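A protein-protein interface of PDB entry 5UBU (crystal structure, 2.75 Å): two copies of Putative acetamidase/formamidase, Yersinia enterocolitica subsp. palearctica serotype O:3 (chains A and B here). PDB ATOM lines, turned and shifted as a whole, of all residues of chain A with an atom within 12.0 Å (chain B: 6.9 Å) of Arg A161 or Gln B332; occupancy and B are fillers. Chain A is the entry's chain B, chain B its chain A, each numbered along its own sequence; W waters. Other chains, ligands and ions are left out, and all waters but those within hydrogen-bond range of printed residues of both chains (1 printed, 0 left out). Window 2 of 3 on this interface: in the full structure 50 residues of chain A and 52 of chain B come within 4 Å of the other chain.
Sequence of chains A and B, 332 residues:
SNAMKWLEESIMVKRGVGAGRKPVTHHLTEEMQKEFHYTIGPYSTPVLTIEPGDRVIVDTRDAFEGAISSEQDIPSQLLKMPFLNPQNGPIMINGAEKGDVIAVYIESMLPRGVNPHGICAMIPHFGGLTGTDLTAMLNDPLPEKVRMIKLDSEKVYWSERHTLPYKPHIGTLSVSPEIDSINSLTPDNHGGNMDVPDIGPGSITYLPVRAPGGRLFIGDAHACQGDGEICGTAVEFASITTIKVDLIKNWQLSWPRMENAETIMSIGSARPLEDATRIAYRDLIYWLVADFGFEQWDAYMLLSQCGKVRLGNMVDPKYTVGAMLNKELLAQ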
ATOM      1  N   ARG A 147     -29.879  -4.362  25.810  1.00  0.00           N
ATOM      2  CA  ARG A 147     -29.597  -3.941  24.450  1.00  0.00           C
ATOM      3  C   ARG A 147     -30.870  -4.077  23.628  1.00  0.00           C
ATOM      4  O   ARG A 147     -31.459  -5.144  23.605  1.00  0.00           O
ATOM      5  CB  ARG A 147     -28.510  -4.799  23.838  1.00  0.00           C
ATOM      6  CG  ARG A 147     -27.113  -4.606  24.399  1.00  0.00           C
ATOM      7  CD  ARG A 147     -26.547  -3.202  24.164  1.00  0.00           C
ATOM      8  NE  ARG A 147     -27.019  -2.617  22.906  1.00  0.00           N
ATOM      9  CZ  ARG A 147     -26.550  -2.888  21.685  1.00  0.00           C
ATOM     10  NH1 ARG A 147     -25.575  -3.767  21.491  1.00  0.00           N
ATOM     11  NH2 ARG A 147     -27.074  -2.270  20.629  1.00  0.00           N
ATOM     12  N   ILE A 149     -32.058  -4.192  20.098  1.00  0.00           N
ATOM     13  CA  ILE A 149     -31.493  -4.430  18.786  1.00  0.00           C
ATOM     14  C   ILE A 149     -32.554  -4.407  17.703  1.00  0.00           C
ATOM     15  O   ILE A 149     -33.539  -5.128  17.760  1.00  0.00           O
ATOM     16  CB  ILE A 149     -30.785  -5.817  18.727  1.00  0.00           C
ATOM     17  CG1 ILE A 149     -29.835  -6.018  19.915  1.00  0.00           C
ATOM     18  CG2 ILE A 149     -30.101  -6.019  17.382  1.00  0.00           C
ATOM     19  CD1 ILE A 149     -28.951  -4.834  20.184  1.00  0.00           C
ATOM     20  N   LYS A 155     -31.249  -9.611   8.816  1.00  0.00           N
ATOM     21  CA  LYS A 155     -30.140  -9.321   9.745  1.00  0.00           C
ATOM     22  C   LYS A 155     -30.538  -8.793  11.131  1.00  0.00           C
ATOM     23  O   LYS A 155     -31.636  -8.285  11.326  1.00  0.00           O
ATOM     24  CB  LYS A 155     -29.213  -8.283   9.085  1.00  0.00           C
ATOM     25  CG  LYS A 155     -28.606  -8.774   7.770  1.00  0.00           C
ATOM     26  CD  LYS A 155     -27.737  -7.805   7.023  1.00  0.00           C
ATOM     27  CE  LYS A 155     -27.194  -8.524   5.787  1.00  0.00           C
ATOM     28  NZ  LYS A 155     -26.363  -7.686   4.870  1.00  0.00           N
ATOM     29  N   VAL A 156     -29.604  -8.927  12.076  1.00  0.00           N
ATOM     30  CA  VAL A 156     -29.749  -8.461  13.462  1.00  0.00           C
ATOM     31  C   VAL A 156     -28.694  -7.368  13.629  1.00  0.00           C
ATOM     32  O   VAL A 156     -27.498  -7.648  13.606  1.00  0.00           O
ATOM     33  CB  VAL A 156     -29.522  -9.595  14.473  1.00  0.00           C
ATOM     34  CG1 VAL A 156     -29.659  -9.078  15.901  1.00  0.00           C
ATOM     35  CG2 VAL A 156     -30.504 -10.743  14.219  1.00  0.00           C
ATOM     36  N   TYR A 157     -29.143  -6.125  13.791  1.00  0.00           N
ATOM     37  CA  TYR A 157     -28.242  -4.969  13.877  1.00  0.00           C
ATOM     38  C   TYR A 157     -27.682  -4.734  15.273  1.00  0.00           C
ATOM     39  O   TYR A 157     -28.005  -3.742  15.929  1.00  0.00           O
ATOM     40  CB  TYR A 157     -28.966  -3.728  13.338  1.00  0.00           C
ATOM     41  CG  TYR A 157     -29.458  -3.945  11.928  1.00  0.00           C
ATOM     42  CD1 TYR A 157     -28.602  -3.793  10.837  1.00  0.00           C
ATOM     43  CD2 TYR A 157     -30.770  -4.339  11.680  1.00  0.00           C
ATOM     44  CE1 TYR A 157     -29.041  -4.014   9.543  1.00  0.00           C
ATOM     45  CE2 TYR A 157     -31.224  -4.550  10.383  1.00  0.00           C
ATOM     46  CZ  TYR A 157     -30.353  -4.388   9.322  1.00  0.00           C
ATOM     47  OH  TYR A 157     -30.791  -4.598   8.048  1.00  0.00           O
ATOM     48  N   TRP A 158     -26.804  -5.646  15.693  1.00  0.00           N
ATOM     49  CA  TRP A 158     -26.186  -5.606  17.020  1.00  0.00           C
ATOM     50  C   TRP A 158     -25.476  -4.289  17.327  1.00  0.00           C
ATOM     51  O   TRP A 158     -25.643  -3.735  18.409  1.00  0.00           O
ATOM     52  CB  TRP A 158     -25.200  -6.772  17.195  1.00  0.00           C
ATOM     53  CG  TRP A 158     -24.640  -6.849  18.566  1.00  0.00           C
ATOM     54  CD1 TRP A 158     -23.462  -6.322  19.010  1.00  0.00           C
ATOM     55  CD2 TRP A 158     -25.263  -7.458  19.695  1.00  0.00           C
ATOM     56  NE1 TRP A 158     -23.308  -6.582  20.351  1.00  0.00           N
ATOM     57  CE2 TRP A 158     -24.401  -7.281  20.794  1.00  0.00           C
ATOM     58  CE3 TRP A 158     -26.469  -8.142  19.885  1.00  0.00           C
ATOM     59  CZ2 TRP A 158     -24.706  -7.765  22.064  1.00  0.00           C
ATOM     60  CZ3 TRP A 158     -26.767  -8.632  21.144  1.00  0.00           C
ATOM     61  CH2 TRP A 158     -25.892  -8.439  22.217  1.00  0.00           C
ATOM     62  N   SER A 159     -24.669  -3.819  16.379  1.00  0.00           N
ATOM     63  CA  SER A 159     -23.925  -2.569  16.541  1.00  0.00           C
ATOM     64  C   SER A 159     -23.301  -2.126  15.217  1.00  0.00           C
ATOM     65  O   SER A 159     -23.402  -2.829  14.213  1.00  0.00           O
ATOM     66  CB  SER A 159     -22.809  -2.751  17.581  1.00  0.00           C
ATOM     67  OG  SER A 159     -21.875  -3.740  17.171  1.00  0.00           O
ATOM     68  N   GLU A 160     -22.660  -0.954  15.222  1.00  0.00           N
ATOM     69  CA  GLU A 160     -21.958  -0.453  14.041  1.00  0.00           C
ATOM     70  C   GLU A 160     -20.962  -1.495  13.544  1.00  0.00           C
ATOM     71  O   GLU A 160     -20.872  -1.782  12.355  1.00  0.00           O
ATOM     72  CB  GLU A 160     -21.197   0.831  14.396  1.00  0.00           C
ATOM     73  CG  GLU A 160     -22.089   2.066  14.487  1.00  0.00           C
ATOM     74  CD  GLU A 160     -22.368   2.672  13.114  1.00  0.00           C
ATOM     75  OE1 GLU A 160     -21.375   2.921  12.381  1.00  0.00           O
ATOM     76  OE2 GLU A 160     -23.556   2.940  12.785  1.00  0.00           O
ATOM     77  N   ARG A 161     -20.236  -2.061  14.501  1.00  0.00           N
ATOM     78  CA  ARG A 161     -19.207  -3.047  14.221  1.00  0.00           C
ATOM     79  C   ARG A 161     -19.736  -4.425  13.814  1.00  0.00           C
ATOM     80  O   ARG A 161     -19.173  -5.054  12.916  1.00  0.00           O
ATOM     81  CB  ARG A 161     -18.292  -3.181  15.441  1.00  0.00           C
ATOM     82  CG  ARG A 161     -17.124  -4.126  15.238  1.00  0.00           C
ATOM     83  CD  ARG A 161     -16.230  -4.168  16.456  1.00  0.00           C
ATOM     84  NE  ARG A 161     -15.083  -5.039  16.230  1.00  0.00           N
ATOM     85  CZ  ARG A 161     -14.124  -5.278  17.124  1.00  0.00           C
ATOM     86  NH1 ARG A 161     -13.119  -6.102  16.820  1.00  0.00           N
ATOM     87  NH2 ARG A 161     -14.165  -4.703  18.324  1.00  0.00           N
ATOM     88  N   HIS A 162     -20.796  -4.897  14.473  1.00  0.00           N
ATOM     89  CA  HIS A 162     -21.340  -6.237  14.182  1.00  0.00           C
ATOM     90  C   HIS A 162     -22.791  -6.285  13.734  1.00  0.00           C
ATOM     91  O   HIS A 162     -23.680  -5.789  14.421  1.00  0.00           O
ATOM     92  CB  HIS A 162     -21.191  -7.152  15.402  1.00  0.00           C
ATOM     93  CG  HIS A 162     -19.780  -7.309  15.863  1.00  0.00           C
ATOM     94  ND1 HIS A 162     -19.276  -6.641  16.958  1.00  0.00           N
ATOM     95  CD2 HIS A 162     -18.753  -8.023  15.350  1.00  0.00           C
ATOM     96  CE1 HIS A 162     -18.006  -6.962  17.118  1.00  0.00           C
ATOM     97  NE2 HIS A 162     -17.662  -7.795  16.151  1.00  0.00           N
ATOM     98  N   THR A 163     -22.998  -6.886  12.562  1.00  0.00           N
ATOM     99  CA  THR A 163     -24.322  -7.095  11.992  1.00  0.00           C
ATOM    100  C   THR A 163     -24.378  -8.605  11.875  1.00  0.00           C
ATOM    101  O   THR A 163     -23.605  -9.198  11.127  1.00  0.00           O
ATOM    102  CB  THR A 163     -24.487  -6.412  10.625  1.00  0.00           C
ATOM    103  OG1 THR A 163     -24.347  -4.999  10.789  1.00  0.00           O
ATOM    104  CG2 THR A 163     -25.875  -6.694  10.053  1.00  0.00           C
ATOM    105  N   LEU A 164     -25.262  -9.227  12.645  1.00  0.00           N
ATOM    106  CA  LEU A 164     -25.375 -10.685  12.663  1.00  0.00           C
ATOM    107  C   LEU A 164     -26.473 -11.193  11.735  1.00  0.00           C
ATOM    108  O   LEU A 164     -27.480 -10.499  11.529  1.00  0.00           O
ATOM    109  CB  LEU A 164     -25.686 -11.155  14.078  1.00  0.00           C
ATOM    110  CG  LEU A 164     -24.787 -10.612  15.179  1.00  0.00           C
ATOM    111  CD1 LEU A 164     -25.269 -11.142  16.523  1.00  0.00           C
ATOM    112  CD2 LEU A 164     -23.328 -10.968  14.888  1.00  0.00           C
ATOM    113  N   PRO A 165     -26.288 -12.400  11.160  1.00  0.00           N
ATOM    114  CA  PRO A 165     -27.356 -12.930  10.317  1.00  0.00           C
ATOM    115  C   PRO A 165     -28.570 -13.318  11.157  1.00  0.00           C
ATOM    116  O   PRO A 165     -28.438 -13.669  12.329  1.00  0.00           O
ATOM    117  CB  PRO A 165     -26.733 -14.182   9.682  1.00  0.00           C
ATOM    118  CG  PRO A 165     -25.266 -14.011   9.826  1.00  0.00           C
ATOM    119  CD  PRO A 165     -25.071 -13.225  11.088  1.00  0.00           C
ATOM    120  N   LEU B 288     -10.622 -11.335  23.478  1.00  0.00           N
ATOM    121  CA  LEU B 288     -11.296 -10.345  22.636  1.00  0.00           C
ATOM    122  C   LEU B 288     -11.088  -8.922  23.160  1.00  0.00           C
ATOM    123  O   LEU B 288     -10.935  -7.990  22.376  1.00  0.00           O
ATOM    124  CB  LEU B 288     -12.788 -10.668  22.515  1.00  0.00           C
ATOM    125  CG  LEU B 288     -13.122 -11.984  21.805  1.00  0.00           C
ATOM    126  CD1 LEU B 288     -14.604 -12.299  21.928  1.00  0.00           C
ATOM    127  CD2 LEU B 288     -12.687 -11.981  20.349  1.00  0.00           C
ATOM    128  N   ASP B 291      -6.764  -8.178  22.754  1.00  0.00           N
ATOM    129  CA  ASP B 291      -6.223  -8.059  21.393  1.00  0.00           C
ATOM    130  C   ASP B 291      -7.162  -7.616  20.266  1.00  0.00           C
ATOM    131  O   ASP B 291      -6.675  -7.266  19.186  1.00  0.00           O
ATOM    132  CB  ASP B 291      -5.628  -9.415  20.974  1.00  0.00           C
ATOM    133  CG  ASP B 291      -4.500  -9.886  21.888  1.00  0.00           C
ATOM    134  OD1 ASP B 291      -4.030  -9.106  22.736  1.00  0.00           O
ATOM    135  OD2 ASP B 291      -4.092 -11.059  21.721  1.00  0.00           O
ATOM    136  N   PHE B 292      -8.476  -7.625  20.481  1.00  0.00           N
ATOM    137  CA  PHE B 292      -9.405  -7.260  19.401  1.00  0.00           C
ATOM    138  C   PHE B 292     -10.360  -6.088  19.696  1.00  0.00           C
ATOM    139  O   PHE B 292     -11.458  -6.008  19.125  1.00  0.00           O
ATOM    140  CB  PHE B 292     -10.166  -8.519  18.940  1.00  0.00           C
ATOM    141  CG  PHE B 292      -9.264  -9.638  18.491  1.00  0.00           C
ATOM    142  CD1 PHE B 292      -8.723  -9.644  17.210  1.00  0.00           C
ATOM    143  CD2 PHE B 292      -8.945 -10.682  19.346  1.00  0.00           C
ATOM    144  CE1 PHE B 292      -7.888 -10.673  16.792  1.00  0.00           C
ATOM    145  CE2 PHE B 292      -8.113 -11.717  18.932  1.00  0.00           C
ATOM    146  CZ  PHE B 292      -7.585 -11.712  17.658  1.00  0.00           C
ATOM    147  N   GLY B 293      -9.934  -5.182  20.573  1.00  0.00           N
ATOM    148  CA  GLY B 293     -10.706  -3.979  20.908  1.00  0.00           C
ATOM    149  C   GLY B 293     -12.134  -4.075  21.421  1.00  0.00           C
ATOM    150  O   GLY B 293     -12.879  -3.096  21.352  1.00  0.00           O
ATOM    151  N   PHE B 294     -12.532  -5.234  21.932  1.00  0.00           N
ATOM    152  CA  PHE B 294     -13.880  -5.386  22.478  1.00  0.00           C
ATOM    153  C   PHE B 294     -13.995  -4.807  23.879  1.00  0.00           C
ATOM    154  O   PHE B 294     -13.019  -4.750  24.626  1.00  0.00           O
ATOM    155  CB  PHE B 294     -14.279  -6.864  22.569  1.00  0.00           C
ATOM    156  CG  PHE B 294     -14.700  -7.477  21.265  1.00  0.00           C
ATOM    157  CD1 PHE B 294     -13.762  -7.900  20.339  1.00  0.00           C
ATOM    158  CD2 PHE B 294     -16.048  -7.684  20.993  1.00  0.00           C
ATOM    159  CE1 PHE B 294     -14.156  -8.495  19.150  1.00  0.00           C
ATOM    160  CE2 PHE B 294     -16.453  -8.277  19.808  1.00  0.00           C
ATOM    161  CZ  PHE B 294     -15.506  -8.678  18.878  1.00  0.00           C
ATOM    162  N   GLU B 295     -15.201  -4.359  24.215  1.00  0.00           N
ATOM    163  CA  GLU B 295     -15.517  -3.889  25.555  1.00  0.00           C
ATOM    164  C   GLU B 295     -16.002  -5.195  26.202  1.00  0.00           C
ATOM    165  O   GLU B 295     -16.687  -5.985  25.551  1.00  0.00           O
ATOM    166  CB  GLU B 295     -16.565  -2.769  25.516  1.00  0.00           C
ATOM    167  CG  GLU B 295     -16.979  -2.206  26.877  1.00  0.00           C
ATOM    168  CD  GLU B 295     -17.985  -3.070  27.623  1.00  0.00           C
ATOM    169  OE1 GLU B 295     -18.964  -3.552  26.997  1.00  0.00           O
ATOM    170  OE2 GLU B 295     -17.833  -3.230  28.854  1.00  0.00           O
ATOM    171  N   ASP B 298     -19.881  -6.161  26.179  1.00  0.00           N
ATOM    172  CA  ASP B 298     -20.365  -6.311  24.811  1.00  0.00           C
ATOM    173  C   ASP B 298     -19.911  -7.668  24.286  1.00  0.00           C
ATOM    174  O   ASP B 298     -20.684  -8.369  23.645  1.00  0.00           O
ATOM    175  CB  ASP B 298     -19.828  -5.208  23.895  1.00  0.00           C
ATOM    176  CG  ASP B 298     -20.362  -5.319  22.477  1.00  0.00           C
ATOM    177  OD1 ASP B 298     -21.597  -5.437  22.300  1.00  0.00           O
ATOM    178  OD2 ASP B 298     -19.543  -5.259  21.538  1.00  0.00           O
ATOM    179  N   GLU B 328     -14.438 -13.577  10.994  1.00  0.00           N
ATOM    180  CA  GLU B 328     -15.156 -12.467  10.365  1.00  0.00           C
ATOM    181  C   GLU B 328     -15.665 -11.471  11.412  1.00  0.00           C
ATOM    182  O   GLU B 328     -15.709 -10.273  11.155  1.00  0.00           O
ATOM    183  CB  GLU B 328     -16.310 -12.969   9.497  1.00  0.00           C
ATOM    184  CG  GLU B 328     -15.857 -13.615   8.195  1.00  0.00           C
ATOM    185  CD  GLU B 328     -17.020 -14.057   7.310  1.00  0.00           C
ATOM    186  OE1 GLU B 328     -16.909 -13.919   6.068  1.00  0.00           O
ATOM    187  OE2 GLU B 328     -18.060 -14.515   7.847  1.00  0.00           O
ATOM    188  N   LEU B 329     -16.010 -11.968  12.595  1.00  0.00           N
ATOM    189  CA  LEU B 329     -16.515 -11.122  13.683  1.00  0.00           C
ATOM    190  C   LEU B 329     -15.401 -10.384  14.457  1.00  0.00           C
ATOM    191  O   LEU B 329     -15.691  -9.634  15.395  1.00  0.00           O
ATOM    192  CB  LEU B 329     -17.403 -11.942  14.628  1.00  0.00           C
ATOM    193  CG  LEU B 329     -18.634 -12.588  13.965  1.00  0.00           C
ATOM    194  CD1 LEU B 329     -19.356 -13.526  14.923  1.00  0.00           C
ATOM    195  CD2 LEU B 329     -19.600 -11.549  13.416  1.00  0.00           C
ATOM    196  N   LEU B 330     -14.138 -10.603  14.070  1.00  0.00           N
ATOM    197  CA  LEU B 330     -12.990  -9.919  14.686  1.00  0.00           C
ATOM    198  C   LEU B 330     -12.692  -8.595  13.968  1.00  0.00           C
ATOM    199  O   LEU B 330     -11.936  -7.771  14.486  1.00  0.00           O
ATOM    200  CB  LEU B 330     -11.734 -10.806  14.664  1.00  0.00           C
ATOM    201  CG  LEU B 330     -11.792 -12.138  15.401  1.00  0.00           C
ATOM    202  CD1 LEU B 330     -10.502 -12.915  15.190  1.00  0.00           C
ATOM    203  CD2 LEU B 330     -12.047 -11.915  16.877  1.00  0.00           C
ATOM    204  N   ALA B 331     -13.271  -8.414  12.774  1.00  0.00           N
ATOM    205  CA  ALA B 331     -13.085  -7.192  11.985  1.00  0.00           C
ATOM    206  C   ALA B 331     -13.464  -5.975  12.816  1.00  0.00           C
ATOM    207  O   ALA B 331     -14.477  -5.985  13.521  1.00  0.00           O
ATOM    208  CB  ALA B 331     -13.917  -7.244  10.710  1.00  0.00           C
ATOM    209  N   GLN B 332     -12.617  -4.948  12.742  1.00  0.00           N
ATOM    210  CA  GLN B 332     -12.806  -3.722  13.513  1.00  0.00           C
ATOM    211  C   GLN B 332     -13.961  -2.882  12.914  1.00  0.00           C
ATOM    212  O   GLN B 332     -14.485  -3.154  11.820  1.00  0.00           O
ATOM    213  CB  GLN B 332     -11.490  -2.923  13.549  1.00  0.00           C
ATOM    214  CG  GLN B 332     -11.357  -1.955  14.727  1.00  0.00           C
ATOM    215  CD  GLN B 332     -11.103  -2.647  16.074  1.00  0.00           C
ATOM    216  OE1 GLN B 332     -11.734  -2.310  17.084  1.00  0.00           O
ATOM    217  NE2 GLN B 332     -10.187  -3.624  16.091  1.00  0.00           N
ATOM    218  OXT GLN B 332     -14.414  -1.916  13.534  1.00  0.00           O
HETATM  219  O   HOH W   1     -20.155  -4.900  18.981  1.00  0.00           O
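Among the printed residues, merely in contact across the chains: His A162 with Phe B294 (3.4 Å), Arg A161 with Phe B294 (3.5 Å), Arg A161 with Gln B332 (3.6 Å) and Arg A161 with Gly B293 (3.7 Å).
Lys A155 touches none of the printed residues of chain B. Glu A160 touches none of the printed residues of chain B. Of chain B, only Phe B292, Gly B293, Phe B294, Leu B330, Ala B331 and Gln B332 come within 4 Å of Arg A161. Printed residues of chain B within 4 Å of His A162: Phe B294 and Leu B329. Of chain A, only Arg A161 comes within 4 Å of Phe B292. Of chain A, only Arg A161 comes within 4 Å of Gly B293. Printed residues of chain A within 4 Å of Phe B294: Arg A161 (3.5 Å) and His A162 (3.4 Å). Of the printed residues of chain A, Asp B298 touches Trp A158 (2.8 Å). Of the printed residues of chain A, Leu B330 touches Arg A161. Ala B331 touches just one residue of chain A: Arg A161 (2.9 Å). Gln B332 touches just one residue of chain A: Arg A161. The nearest residue of chain B that does not touch Arg A161 is Leu B329 (4.6 Å).
Water W1 lies within hydrogen-bond range of OD2 of Asp B298 (2.7 Å), OG of Ser A159 (2.8 Å) and ND1 of His A162 (2.8 Å).
No position is printed for both chains.
N of Gly B293 is in hydrogen-bond range of O of Leu B288, at 3.5 Å. N of Phe B294 lies within hydrogen-bond range of O of Leu B288, 3.2 Å away. The backbone NH (N) of Asp B298 sits at hydrogen-bond distance from the side-chain carboxylate (OE1) of Glu B295. The guanidinium group (NH2) of Arg A147 sits at hydrogen-bond distance from the backbone carbonyl oxygen (O) of Trp A158 (3.0 Å). OG of Ser A159 lies within hydrogen-bond range of N of His A162 (3.1 Å).
Of the 12 printed residues of chain B, 8 touch a printed residue of chain A. Printed residues of chain B that touch a printed residue of chain A: Phe B292, Gly B293, Phe B294, Asp B298, Leu B329, Leu B330, Ala B331 and Gln B332. Along chain B the printed residues that touch a printed residue of chain A span positions 292 to 332. Of the 13 printed residues of chain A, 3 touch a printed residue of chain B. Printed residues of chain A that touch a printed residue of chain B: Trp A158, Arg A161 and His A162. Among the printed residues, no Asp or Glu carboxylate lies within 4 Å of a Lys or Arg side-chain nitrogen of the other chain.
O of Phe B292 is in hydrogen-bond range of NH1 of Arg A161, at 2.8 Å. The side-chain carboxylate (OD1) of Asp B298 lies within hydrogen-bond range of the indole nitrogen (NE1) of Trp A158 (2.8 Å). O of Leu B329 lies within hydrogen-bond range of NE2 of His A162, at 2.8 Å. The backbone carbonyl oxygen of Leu B330 lies within hydrogen-bond range of the guanidinium group of Arg A161 (3.1 Å). The guanidinium group (NE) of Arg A161 is in hydrogen-bond range of the backbone carbonyl oxygen (O) of Ala B331.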
